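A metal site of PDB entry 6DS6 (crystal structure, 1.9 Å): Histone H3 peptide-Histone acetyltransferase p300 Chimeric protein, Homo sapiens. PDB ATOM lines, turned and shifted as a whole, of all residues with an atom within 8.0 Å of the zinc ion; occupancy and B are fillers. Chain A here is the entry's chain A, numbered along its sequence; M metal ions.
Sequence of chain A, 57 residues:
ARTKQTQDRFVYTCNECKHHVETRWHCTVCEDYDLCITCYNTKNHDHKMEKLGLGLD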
ATOM      1  N   HIS A  26     -13.208 -16.030  22.841  1.00  0.00           N
ATOM      2  CA  HIS A  26     -13.522 -15.385  24.101  1.00  0.00           C
ATOM      3  C   HIS A  26     -12.268 -15.320  24.962  1.00  0.00           C
ATOM      4  O   HIS A  26     -11.581 -16.331  25.144  1.00  0.00           O
ATOM      5  CB  HIS A  26     -14.635 -16.136  24.828  1.00  0.00           C
ATOM      6  CG  HIS A  26     -15.020 -15.515  26.137  1.00  0.00           C
ATOM      7  ND1 HIS A  26     -15.697 -14.313  26.222  1.00  0.00           N
ATOM      8  CD2 HIS A  26     -14.819 -15.925  27.410  1.00  0.00           C
ATOM      9  CE1 HIS A  26     -15.912 -14.015  27.489  1.00  0.00           C
ATOM     10  NE2 HIS A  26     -15.375 -14.970  28.228  1.00  0.00           N
ATOM     11  N   CYS A  27     -11.969 -14.138  25.487  1.00  0.00           N
ATOM     12  CA  CYS A  27     -10.796 -13.979  26.334  1.00  0.00           C
ATOM     13  C   CYS A  27     -11.054 -14.621  27.689  1.00  0.00           C
ATOM     14  O   CYS A  27     -12.118 -14.435  28.287  1.00  0.00           O
ATOM     15  CB  CYS A  27     -10.442 -12.504  26.502  1.00  0.00           C
ATOM     16  SG  CYS A  27      -8.978 -12.290  27.509  1.00  0.00           S
ATOM     17  N   THR A  28     -10.100 -15.414  28.154  1.00  0.00           N
ATOM     18  CA  THR A  28     -10.234 -16.064  29.456  1.00  0.00           C
ATOM     19  C   THR A  28      -9.865 -15.139  30.605  1.00  0.00           C
ATOM     20  O   THR A  28     -10.083 -15.511  31.766  1.00  0.00           O
ATOM     21  CB  THR A  28      -9.366 -17.323  29.520  1.00  0.00           C
ATOM     22  OG1 THR A  28      -7.980 -16.948  29.375  1.00  0.00           O
ATOM     23  CG2 THR A  28      -9.745 -18.286  28.387  1.00  0.00           C
ATOM     24  N   VAL A  29      -9.348 -13.952  30.310  1.00  0.00           N
ATOM     25  CA  VAL A  29      -8.780 -13.040  31.293  1.00  0.00           C
ATOM     26  C   VAL A  29      -9.622 -11.777  31.437  1.00  0.00           C
ATOM     27  O   VAL A  29     -10.011 -11.416  32.543  1.00  0.00           O
ATOM     28  CB  VAL A  29      -7.319 -12.686  30.921  1.00  0.00           C
ATOM     29  CG1 VAL A  29      -6.779 -11.621  31.855  1.00  0.00           C
ATOM     30  CG2 VAL A  29      -6.453 -13.954  30.945  1.00  0.00           C
ATOM     31  N   CYS A  30      -9.875 -11.085  30.331  1.00  0.00           N
ATOM     32  CA  CYS A  30     -10.783  -9.945  30.372  1.00  0.00           C
ATOM     33  C   CYS A  30     -12.146 -10.394  30.838  1.00  0.00           C
ATOM     34  O   CYS A  30     -12.502 -11.573  30.768  1.00  0.00           O
ATOM     35  CB  CYS A  30     -10.865  -9.273  28.990  1.00  0.00           C
ATOM     36  SG  CYS A  30      -9.284  -8.480  28.442  1.00  0.00           S
ATOM     37  N   GLU A  31     -12.920  -9.447  31.358  1.00  0.00           N
ATOM     38  CA  GLU A  31     -14.270  -9.789  31.788  1.00  0.00           C
ATOM     39  C   GLU A  31     -15.209  -9.916  30.604  1.00  0.00           C
ATOM     40  O   GLU A  31     -16.099 -10.777  30.617  1.00  0.00           O
ATOM     41  CB  GLU A  31     -14.805  -8.737  32.773  1.00  0.00           C
ATOM     42  CG  GLU A  31     -16.081  -9.177  33.482  1.00  0.00           C
ATOM     43  CD  GLU A  31     -17.193  -8.157  33.375  1.00  0.00           C
ATOM     44  OE1 GLU A  31     -16.885  -6.947  33.230  1.00  0.00           O
ATOM     45  OE2 GLU A  31     -18.375  -8.568  33.431  1.00  0.00           O
ATOM     46  N   ASP A  32     -15.021  -9.108  29.575  1.00  0.00           N
ATOM     47  CA  ASP A  32     -16.038  -8.955  28.535  1.00  0.00           C
ATOM     48  C   ASP A  32     -15.448  -8.726  27.158  1.00  0.00           C
ATOM     49  O   ASP A  32     -15.872  -7.821  26.427  1.00  0.00           O
ATOM     50  CB  ASP A  32     -16.966  -7.791  28.915  1.00  0.00           C
ATOM     51  CG  ASP A  32     -18.214  -7.741  28.068  1.00  0.00           C
ATOM     52  OD1 ASP A  32     -18.680  -8.821  27.661  1.00  0.00           O
ATOM     53  OD2 ASP A  32     -18.733  -6.638  27.813  1.00  0.00           O
ATOM     54  N   TYR A  33     -14.471  -9.544  26.748  1.00  0.00           N
ATOM     55  CA  TYR A  33     -13.757  -9.326  25.494  1.00  0.00           C
ATOM     56  C   TYR A  33     -13.951 -10.515  24.573  1.00  0.00           C
ATOM     57  O   TYR A  33     -13.584 -11.649  24.919  1.00  0.00           O
ATOM     58  CB  TYR A  33     -12.267  -9.057  25.755  1.00  0.00           C
ATOM     59  CG  TYR A  33     -11.534  -8.513  24.554  1.00  0.00           C
ATOM     60  CD1 TYR A  33     -11.457  -7.138  24.319  1.00  0.00           C
ATOM     61  CD2 TYR A  33     -10.923  -9.371  23.642  1.00  0.00           C
ATOM     62  CE1 TYR A  33     -10.791  -6.633  23.208  1.00  0.00           C
ATOM     63  CE2 TYR A  33     -10.259  -8.882  22.527  1.00  0.00           C
ATOM     64  CZ  TYR A  33     -10.187  -7.509  22.325  1.00  0.00           C
ATOM     65  OH  TYR A  33      -9.530  -7.045  21.221  1.00  0.00           O
ATOM     66  N   ASP A  34     -14.502 -10.265  23.380  1.00  0.00           N
ATOM     67  CA  ASP A  34     -14.685 -11.285  22.363  1.00  0.00           C
ATOM     68  C   ASP A  34     -14.175 -10.769  21.016  1.00  0.00           C
ATOM     69  O   ASP A  34     -14.214  -9.571  20.742  1.00  0.00           O
ATOM     70  CB  ASP A  34     -16.163 -11.704  22.258  1.00  0.00           C
ATOM     71  CG  ASP A  34     -16.717 -12.217  23.567  1.00  0.00           C
ATOM     72  OD1 ASP A  34     -16.557 -13.418  23.851  1.00  0.00           O
ATOM     73  OD2 ASP A  34     -17.288 -11.408  24.350  1.00  0.00           O
ATOM     74  N   HIS A  45      -5.233 -10.853  20.451  1.00  0.00           N
ATOM     75  CA  HIS A  45      -5.311 -10.340  21.807  1.00  0.00           C
ATOM     76  C   HIS A  45      -4.251 -11.001  22.683  1.00  0.00           C
ATOM     77  O   HIS A  45      -4.036 -12.214  22.603  1.00  0.00           O
ATOM     78  CB  HIS A  45      -6.701 -10.640  22.347  1.00  0.00           C
ATOM     79  CG  HIS A  45      -7.068  -9.960  23.619  1.00  0.00           C
ATOM     80  ND1 HIS A  45      -7.209  -8.603  23.728  1.00  0.00           N
ATOM     81  CD2 HIS A  45      -7.359 -10.470  24.836  1.00  0.00           C
ATOM     82  CE1 HIS A  45      -7.563  -8.299  24.961  1.00  0.00           C
ATOM     83  NE2 HIS A  45      -7.657  -9.415  25.661  1.00  0.00           N
ATOM     84  N   ASP A  46      -3.613 -10.205  23.547  1.00  0.00           N
ATOM     85  CA  ASP A  46      -2.447 -10.687  24.295  1.00  0.00           C
ATOM     86  C   ASP A  46      -2.833 -11.417  25.570  1.00  0.00           C
ATOM     87  O   ASP A  46      -2.169 -11.294  26.595  1.00  0.00           O
ATOM     88  CB  ASP A  46      -1.508  -9.508  24.593  1.00  0.00           C
ATOM     89  CG  ASP A  46      -0.109  -9.950  25.022  1.00  0.00           C
ATOM     90  OD1 ASP A  46       0.463 -10.886  24.405  1.00  0.00           O
ATOM     91  OD2 ASP A  46       0.422  -9.362  25.982  1.00  0.00           O
ATOM     92  N   HIS A  47      -3.920 -12.192  25.499  1.00  0.00           N
ATOM     93  CA  HIS A  47      -4.358 -13.105  26.556  1.00  0.00           C
ATOM     94  C   HIS A  47      -4.756 -14.434  25.924  1.00  0.00           C
ATOM     95  O   HIS A  47      -5.130 -14.497  24.752  1.00  0.00           O
ATOM     96  CB  HIS A  47      -5.577 -12.594  27.338  1.00  0.00           C
ATOM     97  CG  HIS A  47      -5.301 -11.461  28.268  1.00  0.00           C
ATOM     98  ND1 HIS A  47      -6.159 -10.393  28.410  1.00  0.00           N
ATOM     99  CD2 HIS A  47      -4.270 -11.239  29.120  1.00  0.00           C
ATOM    100  CE1 HIS A  47      -5.670  -9.555  29.300  1.00  0.00           C
ATOM    101  NE2 HIS A  47      -4.524 -10.040  29.752  1.00  0.00           N
ATOM    102  N   LYS A  48      -4.724 -15.482  26.746  1.00  0.00           N
ATOM    103  CA  LYS A  48      -5.272 -16.765  26.336  1.00  0.00           C
ATOM    104  C   LYS A  48      -6.755 -16.618  26.033  1.00  0.00           C
ATOM    105  O   LYS A  48      -7.496 -15.942  26.754  1.00  0.00           O
ATOM    106  CB  LYS A  48      -5.057 -17.822  27.416  1.00  0.00           C
ATOM    107  CG  LYS A  48      -3.716 -18.535  27.325  1.00  0.00           C
ATOM    108  CD  LYS A  48      -3.465 -19.408  28.545  1.00  0.00           C
ATOM    109  CE  LYS A  48      -4.047 -20.800  28.356  1.00  0.00           C
ATOM    110  NZ  LYS A  48      -3.540 -21.748  29.387  1.00  0.00           N
ATOM    111  N   MET A  49      -7.175 -17.244  24.922  1.00  0.00           N
ATOM    112  CA  MET A  49      -8.525 -17.158  24.392  1.00  0.00           C
ATOM    113  C   MET A  49      -9.084 -18.560  24.177  1.00  0.00           C
ATOM    114  O   MET A  49      -8.339 -19.529  23.993  1.00  0.00           O
ATOM    115  CB  MET A  49      -8.531 -16.371  23.085  1.00  0.00           C
ATOM    116  CG  MET A  49      -8.015 -14.953  23.258  1.00  0.00           C
ATOM    117  SD  MET A  49      -8.572 -13.711  22.125  1.00  0.00           S
ATOM    118  CE  MET A  49      -7.218 -13.486  20.980  1.00  0.00           C
HETATM  119 ZN    ZN M   1      -8.166 -10.181  27.350  1.00  0.00          ZN
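Of the 14 residues printed, 4 come within 4 Å of the zinc ion.
The nearest printed residue that does not touch the zinc ion is Val 29 (4.4 Å).
The zinc ion is bound by NE2 of His 45 (1.9 Å), SG of Cys 27 (2.3 Å), ND1 of His 47 (2.3 Å) and SG of Cys 30 (2.3 Å).
O of Tyr 33 is in hydrogen-bond range of N of Cys 27, at 3.0 Å.
N of Val 29 lies close to SG of Cys 27 (3.3 Å).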
